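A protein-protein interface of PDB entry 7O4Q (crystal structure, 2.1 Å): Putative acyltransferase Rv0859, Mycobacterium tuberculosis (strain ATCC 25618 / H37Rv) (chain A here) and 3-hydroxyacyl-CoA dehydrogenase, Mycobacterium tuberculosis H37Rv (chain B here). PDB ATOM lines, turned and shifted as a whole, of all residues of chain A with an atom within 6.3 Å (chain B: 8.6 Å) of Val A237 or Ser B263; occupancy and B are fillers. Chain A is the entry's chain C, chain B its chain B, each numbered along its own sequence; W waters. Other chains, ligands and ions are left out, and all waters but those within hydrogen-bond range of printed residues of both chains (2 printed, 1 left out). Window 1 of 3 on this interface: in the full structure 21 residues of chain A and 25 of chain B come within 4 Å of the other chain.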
ATOM      1  N   ASN A 141      25.571 -28.223  -8.803  1.00  0.00           N
ATOM      2  CA  ASN A 141      24.463 -28.361  -9.742  1.00  0.00           C
ATOM      3  C   ASN A 141      23.945 -26.993 -10.178  1.00  0.00           C
ATOM      4  O   ASN A 141      23.724 -26.749 -11.371  1.00  0.00           O
ATOM      5  CB  ASN A 141      23.359 -29.197  -9.086  1.00  0.00           C
ATOM      6  CG  ASN A 141      22.166 -29.435  -9.992  1.00  0.00           C
ATOM      7  OD1 ASN A 141      21.590 -28.502 -10.557  1.00  0.00           O
ATOM      8  ND2 ASN A 141      21.771 -30.698 -10.112  1.00  0.00           N
ATOM      9  N   TYR A 142      23.746 -26.089  -9.219  1.00  0.00           N
ATOM     10  CA  TYR A 142      23.219 -24.764  -9.529  1.00  0.00           C
ATOM     11  C   TYR A 142      24.157 -24.005 -10.459  1.00  0.00           C
ATOM     12  O   TYR A 142      23.732 -23.473 -11.491  1.00  0.00           O
ATOM     13  CB  TYR A 142      22.996 -23.992  -8.228  1.00  0.00           C
ATOM     14  CG  TYR A 142      22.215 -22.703  -8.342  1.00  0.00           C
ATOM     15  CD1 TYR A 142      22.839 -21.516  -8.707  1.00  0.00           C
ATOM     16  CD2 TYR A 142      20.860 -22.664  -8.040  1.00  0.00           C
ATOM     17  CE1 TYR A 142      22.131 -20.331  -8.792  1.00  0.00           C
ATOM     18  CE2 TYR A 142      20.143 -21.482  -8.117  1.00  0.00           C
ATOM     19  CZ  TYR A 142      20.783 -20.321  -8.497  1.00  0.00           C
ATOM     20  OH  TYR A 142      20.072 -19.147  -8.579  1.00  0.00           O
ATOM     21  N   MET A 145      24.522 -25.397 -13.987  1.00  0.00           N
ATOM     22  CA  MET A 145      23.234 -25.486 -14.676  1.00  0.00           C
ATOM     23  C   MET A 145      23.020 -26.893 -15.237  1.00  0.00           C
ATOM     24  O   MET A 145      22.881 -27.105 -16.445  1.00  0.00           O
ATOM     25  CB  MET A 145      23.114 -24.417 -15.770  1.00  0.00           C
ATOM     26  CG  MET A 145      22.841 -23.016 -15.230  1.00  0.00           C
ATOM     27  SD  MET A 145      22.651 -21.774 -16.525  1.00  0.00           S
ATOM     28  CE  MET A 145      24.326 -21.708 -17.146  1.00  0.00           C
ATOM     29  N   PHE A 146      23.002 -27.857 -14.316  1.00  0.00           N
ATOM     30  CA  PHE A 146      22.817 -29.255 -14.680  1.00  0.00           C
ATOM     31  C   PHE A 146      21.460 -29.468 -15.338  1.00  0.00           C
ATOM     32  O   PHE A 146      20.435 -28.961 -14.872  1.00  0.00           O
ATOM     33  CB  PHE A 146      22.945 -30.141 -13.438  1.00  0.00           C
ATOM     34  CG  PHE A 146      22.662 -31.597 -13.693  1.00  0.00           C
ATOM     35  CD1 PHE A 146      23.665 -32.442 -14.139  1.00  0.00           C
ATOM     36  CD2 PHE A 146      21.395 -32.122 -13.477  1.00  0.00           C
ATOM     37  CE1 PHE A 146      23.409 -33.782 -14.373  1.00  0.00           C
ATOM     38  CE2 PHE A 146      21.133 -33.458 -13.712  1.00  0.00           C
ATOM     39  CZ  PHE A 146      22.142 -34.291 -14.158  1.00  0.00           C
ATOM     40  N   VAL A 147      21.461 -30.232 -16.424  1.00  0.00           N
ATOM     41  CA  VAL A 147      20.248 -30.573 -17.165  1.00  0.00           C
ATOM     42  C   VAL A 147      20.361 -32.025 -17.613  1.00  0.00           C
ATOM     43  O   VAL A 147      21.417 -32.428 -18.122  1.00  0.00           O
ATOM     44  CB  VAL A 147      20.040 -29.626 -18.361  1.00  0.00           C
ATOM     45  CG1 VAL A 147      19.029 -30.201 -19.329  1.00  0.00           C
ATOM     46  CG2 VAL A 147      19.588 -28.254 -17.888  1.00  0.00           C
ATOM     47  N   LEU A 231      11.134 -34.654 -13.771  1.00  0.00           N
ATOM     48  CA  LEU A 231      11.125 -33.701 -12.675  1.00  0.00           C
ATOM     49  C   LEU A 231      11.055 -32.272 -13.214  1.00  0.00           C
ATOM     50  O   LEU A 231      11.151 -32.026 -14.420  1.00  0.00           O
ATOM     51  CB  LEU A 231      12.358 -33.901 -11.793  1.00  0.00           C
ATOM     52  CG  LEU A 231      12.558 -35.342 -11.309  1.00  0.00           C
ATOM     53  CD1 LEU A 231      13.844 -35.494 -10.507  1.00  0.00           C
ATOM     54  CD2 LEU A 231      11.360 -35.808 -10.496  1.00  0.00           C
ATOM     55  N   GLY A 232      10.888 -31.316 -12.299  1.00  0.00           N
ATOM     56  CA  GLY A 232      10.607 -29.948 -12.667  1.00  0.00           C
ATOM     57  C   GLY A 232      11.831 -29.049 -12.739  1.00  0.00           C
ATOM     58  O   GLY A 232      12.859 -29.304 -12.118  1.00  0.00           O
ATOM     59  N   GLY A 233      11.695 -27.980 -13.525  1.00  0.00           N
ATOM     60  CA  GLY A 233      12.673 -26.918 -13.583  1.00  0.00           C
ATOM     61  C   GLY A 233      13.741 -27.070 -14.645  1.00  0.00           C
ATOM     62  O   GLY A 233      14.400 -26.081 -14.983  1.00  0.00           O
ATOM     63  N   PHE A 234      13.931 -28.274 -15.188  1.00  0.00           N
ATOM     64  CA  PHE A 234      15.074 -28.505 -16.065  1.00  0.00           C
ATOM     65  C   PHE A 234      14.922 -27.801 -17.410  1.00  0.00           C
ATOM     66  O   PHE A 234      15.923 -27.348 -17.980  1.00  0.00           O
ATOM     67  CB  PHE A 234      15.283 -30.004 -16.259  1.00  0.00           C
ATOM     68  CG  PHE A 234      15.892 -30.694 -15.069  1.00  0.00           C
ATOM     69  CD1 PHE A 234      17.050 -30.205 -14.483  1.00  0.00           C
ATOM     70  CD2 PHE A 234      15.311 -31.835 -14.539  1.00  0.00           C
ATOM     71  CE1 PHE A 234      17.619 -30.846 -13.391  1.00  0.00           C
ATOM     72  CE2 PHE A 234      15.870 -32.477 -13.449  1.00  0.00           C
ATOM     73  CZ  PHE A 234      17.024 -31.982 -12.874  1.00  0.00           C
ATOM     74  N   ASP A 235      13.697 -27.701 -17.936  1.00  0.00           N
ATOM     75  CA  ASP A 235      13.489 -26.918 -19.153  1.00  0.00           C
ATOM     76  C   ASP A 235      13.846 -25.454 -18.932  1.00  0.00           C
ATOM     77  O   ASP A 235      14.505 -24.835 -19.775  1.00  0.00           O
ATOM     78  CB  ASP A 235      12.041 -27.038 -19.627  1.00  0.00           C
ATOM     79  CG  ASP A 235      11.791 -28.292 -20.434  1.00  0.00           C
ATOM     80  OD1 ASP A 235      12.656 -29.194 -20.425  1.00  0.00           O
ATOM     81  OD2 ASP A 235      10.730 -28.370 -21.088  1.00  0.00           O
ATOM     82  N   ASP A 236      13.420 -24.891 -17.798  1.00  0.00           N
ATOM     83  CA  ASP A 236      13.719 -23.495 -17.494  1.00  0.00           C
ATOM     84  C   ASP A 236      15.220 -23.254 -17.402  1.00  0.00           C
ATOM     85  O   ASP A 236      15.720 -22.228 -17.876  1.00  0.00           O
ATOM     86  CB  ASP A 236      13.038 -23.089 -16.186  1.00  0.00           C
ATOM     87  CG  ASP A 236      11.551 -23.395 -16.179  1.00  0.00           C
ATOM     88  OD1 ASP A 236      11.188 -24.589 -16.250  1.00  0.00           O
ATOM     89  OD2 ASP A 236      10.747 -22.445 -16.093  1.00  0.00           O
ATOM     90  N   VAL A 237      15.955 -24.192 -16.799  1.00  0.00           N
ATOM     91  CA  VAL A 237      17.400 -24.032 -16.658  1.00  0.00           C
ATOM     92  C   VAL A 237      18.069 -24.001 -18.028  1.00  0.00           C
ATOM     93  O   VAL A 237      18.928 -23.153 -18.301  1.00  0.00           O
ATOM     94  CB  VAL A 237      17.978 -25.147 -15.769  1.00  0.00           C
ATOM     95  CG1 VAL A 237      19.496 -25.076 -15.736  1.00  0.00           C
ATOM     96  CG2 VAL A 237      17.412 -25.044 -14.360  1.00  0.00           C
ATOM     97  N   ALA A 238      17.675 -24.921 -18.914  1.00  0.00           N
ATOM     98  CA  ALA A 238      18.282 -24.982 -20.242  1.00  0.00           C
ATOM     99  C   ALA A 238      18.026 -23.703 -21.029  1.00  0.00           C
ATOM    100  O   ALA A 238      18.921 -23.199 -21.718  1.00  0.00           O
ATOM    101  CB  ALA A 238      17.755 -26.194 -21.009  1.00  0.00           C
ATOM    102  N   LEU A 239      16.812 -23.160 -20.942  1.00  0.00           N
ATOM    103  CA  LEU A 239      16.489 -21.954 -21.693  1.00  0.00           C
ATOM    104  C   LEU A 239      17.086 -20.695 -21.075  1.00  0.00           C
ATOM    105  O   LEU A 239      17.139 -19.661 -21.748  1.00  0.00           O
ATOM    106  CB  LEU A 239      14.972 -21.809 -21.824  1.00  0.00           C
ATOM    107  CG  LEU A 239      14.294 -22.952 -22.587  1.00  0.00           C
ATOM    108  CD1 LEU A 239      12.806 -22.690 -22.773  1.00  0.00           C
ATOM    109  CD2 LEU A 239      14.976 -23.185 -23.930  1.00  0.00           C
ATOM    110  N   GLN A 240      17.535 -20.751 -19.818  1.00  0.00           N
ATOM    111  CA  GLN A 240      18.207 -19.591 -19.241  1.00  0.00           C
ATOM    112  C   GLN A 240      19.575 -19.381 -19.877  1.00  0.00           C
ATOM    113  O   GLN A 240      20.014 -18.238 -20.057  1.00  0.00           O
ATOM    114  CB  GLN A 240      18.329 -19.743 -17.722  1.00  0.00           C
ATOM    115  CG  GLN A 240      17.021 -19.486 -16.984  1.00  0.00           C
ATOM    116  CD  GLN A 240      17.094 -19.821 -15.503  1.00  0.00           C
ATOM    117  OE1 GLN A 240      18.172 -20.062 -14.958  1.00  0.00           O
ATOM    118  NE2 GLN A 240      15.938 -19.844 -14.845  1.00  0.00           N
ATOM    119  N   LYS A 241      20.261 -20.471 -20.229  1.00  0.00           N
ATOM    120  CA  LYS A 241      21.500 -20.349 -20.990  1.00  0.00           C
ATOM    121  C   LYS A 241      21.218 -20.115 -22.470  1.00  0.00           C
ATOM    122  O   LYS A 241      21.792 -19.210 -23.083  1.00  0.00           O
ATOM    123  CB  LYS A 241      22.369 -21.594 -20.801  1.00  0.00           C
ATOM    124  CG  LYS A 241      23.466 -21.706 -21.847  1.00  0.00           C
ATOM    125  CD  LYS A 241      24.566 -22.668 -21.437  1.00  0.00           C
ATOM    126  CE  LYS A 241      25.533 -22.025 -20.455  1.00  0.00           C
ATOM    127  NZ  LYS A 241      26.213 -20.828 -21.025  1.00  0.00           N
ATOM    128  N   TYR A 242      20.330 -20.918 -23.061  1.00  0.00           N
ATOM    129  CA  TYR A 242      19.956 -20.753 -24.467  1.00  0.00           C
ATOM    130  C   TYR A 242      18.748 -19.818 -24.564  1.00  0.00           C
ATOM    131  O   TYR A 242      17.638 -20.196 -24.945  1.00  0.00           O
ATOM    132  CB  TYR A 242      19.695 -22.111 -25.107  1.00  0.00           C
ATOM    133  CG  TYR A 242      20.968 -22.904 -25.293  1.00  0.00           C
ATOM    134  CD1 TYR A 242      21.503 -23.653 -24.251  1.00  0.00           C
ATOM    135  CD2 TYR A 242      21.652 -22.877 -26.500  1.00  0.00           C
ATOM    136  CE1 TYR A 242      22.674 -24.365 -24.414  1.00  0.00           C
ATOM    137  CE2 TYR A 242      22.823 -23.586 -26.672  1.00  0.00           C
ATOM    138  CZ  TYR A 242      23.330 -24.326 -25.626  1.00  0.00           C
ATOM    139  OH  TYR A 242      24.498 -25.030 -25.800  1.00  0.00           O
ATOM    140  N   VAL A 297      25.623 -27.686 -20.676  1.00  0.00           N
ATOM    141  CA  VAL A 297      24.174 -27.613 -20.502  1.00  0.00           C
ATOM    142  C   VAL A 297      23.465 -28.357 -21.626  1.00  0.00           C
ATOM    143  O   VAL A 297      22.586 -29.192 -21.381  1.00  0.00           O
ATOM    144  CB  VAL A 297      23.715 -26.147 -20.411  1.00  0.00           C
ATOM    145  CG1 VAL A 297      22.193 -26.062 -20.425  1.00  0.00           C
ATOM    146  CG2 VAL A 297      24.282 -25.495 -19.155  1.00  0.00           C
ATOM    147  N   ILE B 257      15.595 -37.573  -6.550  1.00  0.00           N
ATOM    148  CA  ILE B 257      14.986 -36.266  -6.784  1.00  0.00           C
ATOM    149  C   ILE B 257      15.907 -35.112  -6.430  1.00  0.00           C
ATOM    150  O   ILE B 257      15.616 -33.967  -6.818  1.00  0.00           O
ATOM    151  CB  ILE B 257      13.653 -36.118  -6.020  1.00  0.00           C
ATOM    152  CG1 ILE B 257      13.903 -36.138  -4.511  1.00  0.00           C
ATOM    153  CG2 ILE B 257      12.678 -37.218  -6.426  1.00  0.00           C
ATOM    154  CD1 ILE B 257      12.664 -35.905  -3.679  1.00  0.00           C
ATOM    155  N   LEU B 258      17.001 -35.369  -5.713  1.00  0.00           N
ATOM    156  CA  LEU B 258      17.910 -34.300  -5.308  1.00  0.00           C
ATOM    157  C   LEU B 258      18.457 -33.470  -6.468  1.00  0.00           C
ATOM    158  O   LEU B 258      18.631 -32.253  -6.281  1.00  0.00           O
ATOM    159  CB  LEU B 258      19.051 -34.905  -4.481  1.00  0.00           C
ATOM    160  CG  LEU B 258      20.043 -33.980  -3.775  1.00  0.00           C
ATOM    161  CD1 LEU B 258      19.324 -33.023  -2.842  1.00  0.00           C
ATOM    162  CD2 LEU B 258      21.059 -34.807  -3.005  1.00  0.00           C
ATOM    163  N   PRO B 259      18.763 -34.025  -7.649  1.00  0.00           N
ATOM    164  CA  PRO B 259      19.237 -33.163  -8.746  1.00  0.00           C
ATOM    165  C   PRO B 259      18.231 -32.116  -9.192  1.00  0.00           C
ATOM    166  O   PRO B 259      18.632 -31.121  -9.808  1.00  0.00           O
ATOM    167  CB  PRO B 259      19.539 -34.161  -9.872  1.00  0.00           C
ATOM    168  CG  PRO B 259      19.846 -35.430  -9.166  1.00  0.00           C
ATOM    169  CD  PRO B 259      18.920 -35.454  -7.987  1.00  0.00           C
ATOM    170  N   SER B 260      16.945 -32.298  -8.905  1.00  0.00           N
ATOM    171  CA  SER B 260      15.942 -31.328  -9.322  1.00  0.00           C
ATOM    172  C   SER B 260      15.748 -30.197  -8.319  1.00  0.00           C
ATOM    173  O   SER B 260      15.001 -29.258  -8.612  1.00  0.00           O
ATOM    174  CB  SER B 260      14.597 -32.024  -9.575  1.00  0.00           C
ATOM    175  OG  SER B 260      14.002 -32.460  -8.367  1.00  0.00           O
ATOM    176  N   PHE B 261      16.395 -30.252  -7.149  1.00  0.00           N
ATOM    177  CA  PHE B 261      16.230 -29.160  -6.189  1.00  0.00           C
ATOM    178  C   PHE B 261      16.861 -27.864  -6.686  1.00  0.00           C
ATOM    179  O   PHE B 261      16.199 -26.813  -6.607  1.00  0.00           O
ATOM    180  CB  PHE B 261      16.774 -29.569  -4.814  1.00  0.00           C
ATOM    181  CG  PHE B 261      15.958 -30.626  -4.114  1.00  0.00           C
ATOM    182  CD1 PHE B 261      14.806 -31.141  -4.692  1.00  0.00           C
ATOM    183  CD2 PHE B 261      16.343 -31.098  -2.870  1.00  0.00           C
ATOM    184  CE1 PHE B 261      14.062 -32.114  -4.046  1.00  0.00           C
ATOM    185  CE2 PHE B 261      15.602 -32.067  -2.218  1.00  0.00           C
ATOM    186  CZ  PHE B 261      14.459 -32.577  -2.808  1.00  0.00           C
ATOM    187  N   PRO B 262      18.102 -27.844  -7.194  1.00  0.00           N
ATOM    188  CA  PRO B 262      18.625 -26.579  -7.736  1.00  0.00           C
ATOM    189  C   PRO B 262      17.909 -26.123  -8.996  1.00  0.00           C
ATOM    190  O   PRO B 262      17.784 -24.911  -9.215  1.00  0.00           O
ATOM    191  CB  PRO B 262      20.105 -26.891  -8.009  1.00  0.00           C
ATOM    192  CG  PRO B 262      20.408 -28.086  -7.171  1.00  0.00           C
ATOM    193  CD  PRO B 262      19.146 -28.885  -7.169  1.00  0.00           C
ATOM    194  N   SER B 263      17.439 -27.051  -9.835  1.00  0.00           N
ATOM    195  CA  SER B 263      16.729 -26.645 -11.044  1.00  0.00           C
ATOM    196  C   SER B 263      15.372 -26.042 -10.708  1.00  0.00           C
ATOM    197  O   SER B 263      14.967 -25.038 -11.308  1.00  0.00           O
ATOM    198  CB  SER B 263      16.570 -27.832 -11.993  1.00  0.00           C
ATOM    199  OG  SER B 263      15.730 -28.832 -11.439  1.00  0.00           O
ATOM    200  N   ASN B 264      14.651 -26.640  -9.757  1.00  0.00           N
ATOM    201  CA  ASN B 264      13.408 -26.032  -9.292  1.00  0.00           C
ATOM    202  C   ASN B 264      13.667 -24.661  -8.680  1.00  0.00           C
ATOM    203  O   ASN B 264      12.853 -23.741  -8.834  1.00  0.00           O
ATOM    204  CB  ASN B 264      12.712 -26.953  -8.292  1.00  0.00           C
ATOM    205  CG  ASN B 264      11.929 -28.061  -8.973  1.00  0.00           C
ATOM    206  OD1 ASN B 264      11.169 -27.808  -9.905  1.00  0.00           O
ATOM    207  ND2 ASN B 264      12.126 -29.295  -8.521  1.00  0.00           N
ATOM    208  N   LEU B 265      14.802 -24.502  -7.994  1.00  0.00           N
ATOM    209  CA  LEU B 265      15.172 -23.194  -7.461  1.00  0.00           C
ATOM    210  C   LEU B 265      15.387 -22.187  -8.585  1.00  0.00           C
ATOM    211  O   LEU B 265      14.861 -21.068  -8.541  1.00  0.00           O
ATOM    212  CB  LEU B 265      16.427 -23.314  -6.594  1.00  0.00           C
ATOM    213  CG  LEU B 265      16.886 -22.014  -5.929  1.00  0.00           C
ATOM    214  CD1 LEU B 265      15.781 -21.450  -5.052  1.00  0.00           C
ATOM    215  CD2 LEU B 265      18.154 -22.232  -5.118  1.00  0.00           C
ATOM    216  N   ARG B 266      16.157 -22.570  -9.607  1.00  0.00           N
ATOM    217  CA  ARG B 266      16.369 -21.675 -10.740  1.00  0.00           C
ATOM    218  C   ARG B 266      15.067 -21.373 -11.464  1.00  0.00           C
ATOM    219  O   ARG B 266      14.910 -20.281 -12.021  1.00  0.00           O
ATOM    220  CB  ARG B 266      17.385 -22.272 -11.713  1.00  0.00           C
ATOM    221  CG  ARG B 266      18.790 -22.380 -11.156  1.00  0.00           C
ATOM    222  CD  ARG B 266      19.800 -22.624 -12.263  1.00  0.00           C
ATOM    223  NE  ARG B 266      20.010 -21.424 -13.064  1.00  0.00           N
ATOM    224  CZ  ARG B 266      21.100 -20.668 -13.004  1.00  0.00           C
ATOM    225  NH1 ARG B 266      22.094 -20.992 -12.190  1.00  0.00           N
ATOM    226  NH2 ARG B 266      21.200 -19.590 -13.769  1.00  0.00           N
ATOM    227  N   LYS B 267      14.127 -22.323 -11.476  1.00  0.00           N
ATOM    228  CA  LYS B 267      12.824 -22.064 -12.078  1.00  0.00           C
ATOM    229  C   LYS B 267      12.071 -20.980 -11.313  1.00  0.00           C
ATOM    230  O   LYS B 267      11.472 -20.085 -11.921  1.00  0.00           O
ATOM    231  CB  LYS B 267      12.001 -23.352 -12.130  1.00  0.00           C
ATOM    232  CG  LYS B 267      10.597 -23.166 -12.696  1.00  0.00           C
ATOM    233  CD  LYS B 267       9.787 -24.454 -12.641  1.00  0.00           C
ATOM    234  CE  LYS B 267       8.375 -24.236 -13.162  1.00  0.00           C
ATOM    235  NZ  LYS B 267       7.554 -25.478 -13.103  1.00  0.00           N
ATOM    236  N   GLN B 268      12.094 -21.042  -9.980  1.00  0.00           N
ATOM    237  CA  GLN B 268      11.366 -20.058  -9.184  1.00  0.00           C
ATOM    238  C   GLN B 268      12.057 -18.700  -9.207  1.00  0.00           C
ATOM    239  O   GLN B 268      11.391 -17.660  -9.268  1.00  0.00           O
ATOM    240  CB  GLN B 268      11.209 -20.559  -7.748  1.00  0.00           C
ATOM    241  CG  GLN B 268      10.395 -21.840  -7.628  1.00  0.00           C
ATOM    242  CD  GLN B 268       8.974 -21.680  -8.144  1.00  0.00           C
ATOM    243  OE1 GLN B 268       8.444 -22.561  -8.821  1.00  0.00           O
ATOM    244  NE2 GLN B 268       8.351 -20.553  -7.821  1.00  0.00           N
ATOM    245  N   LEU B 269      13.389 -18.685  -9.165  1.00  0.00           N
ATOM    246  CA  LEU B 269      14.136 -17.434  -9.191  1.00  0.00           C
ATOM    247  C   LEU B 269      14.362 -16.902 -10.600  1.00  0.00           C
ATOM    248  O   LEU B 269      14.768 -15.743 -10.743  1.00  0.00           O
ATOM    249  CB  LEU B 269      15.485 -17.610  -8.488  1.00  0.00           C
ATOM    250  CG  LEU B 269      15.421 -17.886  -6.985  1.00  0.00           C
ATOM    251  CD1 LEU B 269      16.816 -17.906  -6.381  1.00  0.00           C
ATOM    252  CD2 LEU B 269      14.542 -16.858  -6.288  1.00  0.00           C
ATOM    253  N   LYS B 270      14.122 -17.718 -11.627  1.00  0.00           N
ATOM    254  CA  LYS B 270      14.223 -17.321 -13.032  1.00  0.00           C
ATOM    255  C   LYS B 270      15.645 -16.948 -13.434  1.00  0.00           C
ATOM    256  O   LYS B 270      15.848 -16.268 -14.444  1.00  0.00           O
ATOM    257  CB  LYS B 270      13.265 -16.167 -13.359  1.00  0.00           C
ATOM    258  CG  LYS B 270      11.799 -16.474 -13.101  1.00  0.00           C
ATOM    259  CD  LYS B 270      10.916 -15.298 -13.500  1.00  0.00           C
ATOM    260  CE  LYS B 270       9.457 -15.551 -13.156  1.00  0.00           C
ATOM    261  NZ  LYS B 270       8.579 -14.416 -13.565  1.00  0.00           N
ATOM    262  N   GLY B 271      16.638 -17.386 -12.665  1.00  0.00           N
ATOM    263  CA  GLY B 271      18.024 -17.084 -12.953  1.00  0.00           C
ATOM    264  C   GLY B 271      18.525 -15.762 -12.419  1.00  0.00           C
ATOM    265  O   GLY B 271      19.608 -15.323 -12.823  1.00  0.00           O
ATOM    266  N   LEU B 281      20.174 -23.705   0.288  1.00  0.00           N
ATOM    267  CA  LEU B 281      20.046 -25.077  -0.195  1.00  0.00           C
ATOM    268  C   LEU B 281      21.367 -25.830  -0.080  1.00  0.00           C
ATOM    269  O   LEU B 281      21.388 -27.005   0.303  1.00  0.00           O
ATOM    270  CB  LEU B 281      19.543 -25.083  -1.640  1.00  0.00           C
ATOM    271  CG  LEU B 281      19.389 -26.454  -2.308  1.00  0.00           C
ATOM    272  CD1 LEU B 281      18.461 -27.358  -1.506  1.00  0.00           C
ATOM    273  CD2 LEU B 281      18.893 -26.304  -3.740  1.00  0.00           C
ATOM    274  N   GLN B 553      14.037 -13.263 -21.498  1.00  0.00           N
ATOM    275  CA  GLN B 553      14.988 -13.866 -20.568  1.00  0.00           C
ATOM    276  C   GLN B 553      15.806 -12.802 -19.842  1.00  0.00           C
ATOM    277  O   GLN B 553      16.058 -12.920 -18.638  1.00  0.00           O
ATOM    278  CB  GLN B 553      15.909 -14.833 -21.310  1.00  0.00           C
ATOM    279  CG  GLN B 553      15.285 -16.183 -21.620  1.00  0.00           C
ATOM    280  CD  GLN B 553      15.229 -17.095 -20.408  1.00  0.00           C
ATOM    281  OE1 GLN B 553      15.760 -16.770 -19.344  1.00  0.00           O
ATOM    282  NE2 GLN B 553      14.586 -18.248 -20.565  1.00  0.00           N
ATOM    283  N   GLN B 557      15.881 -12.752 -15.870  1.00  0.00           N
ATOM    284  CA  GLN B 557      17.165 -12.979 -15.220  1.00  0.00           C
ATOM    285  C   GLN B 557      17.702 -11.727 -14.541  1.00  0.00           C
ATOM    286  O   GLN B 557      18.519 -11.843 -13.619  1.00  0.00           O
ATOM    287  CB  GLN B 557      18.177 -13.522 -16.233  1.00  0.00           C
ATOM    288  CG  GLN B 557      17.820 -14.916 -16.740  1.00  0.00           C
ATOM    289  CD  GLN B 557      18.860 -15.494 -17.676  1.00  0.00           C
ATOM    290  OE1 GLN B 557      20.060 -15.402 -17.424  1.00  0.00           O
ATOM    291  NE2 GLN B 557      18.402 -16.093 -18.771  1.00  0.00           N
HETATM  292  O   HOH W   1      13.839 -20.283 -18.600  1.00  0.00           O
HETATM  293  O   HOH W   2      18.401 -17.899  -9.910  1.00  0.00           O
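The side-chain hydroxyl (OG) of Ser B260 is in hydrogen-bond range of the backbone carbonyl oxygen (O) of Ile B257 (2.7 Å).
O of Ser B260 sits at hydrogen-bond distance from OG of Ser B263, 3.0 Å away.
The side-chain amide nitrogen (ND2) of Asn B264 is in hydrogen-bond range of the backbone carbonyl oxygen (O) of Ser B260 (2.9 Å).
N of Gly B271 lies within hydrogen-bond range of O of Arg B266, at 3.4 Å.
OE1 of Gln B553 is in hydrogen-bond range of NE2 of Gln B557 (2.8 Å).
The backbone carbonyl oxygen (O) of Asn A141 is in hydrogen-bond range of the backbone NH (N) of Phe A146 (3.2 Å).
O of Pro B259 sits at hydrogen-bond distance from ND2 of Asn A141 (3.2 Å).
OG of Ser B263 sits at hydrogen-bond distance from O of Gly A232 (3.0 Å).
The side-chain amide oxygen (OD1) of Asn B264 sits close to the backbone carbonyl oxygen (O) of Gly A232 (3.2 Å).
The guanidinium group (NH1) of Arg B266 sits at hydrogen-bond distance from the backbone carbonyl oxygen (O) of Tyr A142, at 3.1 Å.
The guanidinium group (NE) of Arg B266 sits at hydrogen-bond distance from the side-chain amide oxygen (OE1) of Gln A240 (3.0 Å).
The backbone NH (N) of Gly B271 lies close to the side-chain amide nitrogen (NE2) of Gln A240 (3.4 Å).
The side-chain amide nitrogen (NE2) of Gln B553 sits at hydrogen-bond distance from the backbone carbonyl oxygen (O) of Leu A239 (3.1 Å).
The side-chain amide nitrogen (NE2) of Gln B557 lies within hydrogen-bond range of the backbone carbonyl oxygen (O) of Gln A240 (3.0 Å).
Val A237 touches just these residues of chain B: Ser B263 and Arg B266.
No residue of chain B comes within 4 Å of Ala A238.
Of the printed residues of chain B, Met A145 touches Arg B266.
Printed residues of chain B within 4 Å of Gln A240: Arg B266 (3.0 Å), Lys B270 (3.2 Å), Gly B271 (3.4 Å), Gln B553 (3.7 Å) and Gln B557 (3.0 Å).
Printed residues of chain A within 4 Å of Pro B259: Asn A141 and Phe A234.
Phe A146 touches none of the printed residues of chain B.
Phe B261 touches none of the printed residues of chain A.
The nearest printed residue of chain B that does not touch Val A237 is Lys B267 (5.1 Å).
The nearest residue of chain A that does not touch Ser B263 is Asn A141 (4.5 Å).
The nearest printed residue of chain B that does not touch Met A145 is Gln B557 (6.9 Å).
Among the printed residues, merely in contact across the chains: Gln A240 with Lys B270 (3.2 Å), Asn A141 with Pro B262 (3.4 Å), Phe A234 with Ser B263 (3.4 Å), Asp A236 with Lys B267 (3.5 Å), Phe A234 with Pro B259 (3.6 Å), Gly A233 with Asn B264 (3.7 Å), Leu A231 with Ser B260 (3.7 Å), Met A145 with Arg B266 (3.7 Å), Tyr A142 with Leu B265 (3.7 Å), Gln A240 with Gln B553 (3.7 Å), Gly A233 with Ser B263 (3.7 Å), Val A237 with Ser B263 (3.7 Å), Phe A234 with Ser B260 (3.8 Å), Val A237 with Arg B266 (3.8 Å), Gly A233 with Lys B267 (3.9 Å), Tyr A142 with Pro B262 (3.9 Å) and Leu A231 with Ile B257 (3.97 Å).
Water W2 lies within hydrogen-bond range of OH of Tyr A142 and N of Gly B271.
Water W1 bridges O of Asp A236 (2.8 Å) and NE2 of Gln B553 (2.9 Å).
Printed residues of chain A that touch a printed residue of chain B: Asn A141, Tyr A142, Met A145, Leu A231, Gly A232, Gly A233, Phe A234, Asp A236, Val A237, Leu A239 and Gln A240.
Along chain A the printed residues that touch a printed residue of chain B span positions 141 to 240.
Of the 18 printed residues of chain B, 13 touch a printed residue of chain A.
Hydrophobic or aromatic side chains of chain B within 4 Å of the printed part of chain A: Pro B262 and Leu B265.
Along chain B the printed residues that touch a printed residue of chain A span positions 257 to 557.
Among the printed residues, no Asp or Glu carboxylate lies within 4 Å of a Lys or Arg side-chain nitrogen of the other chain.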
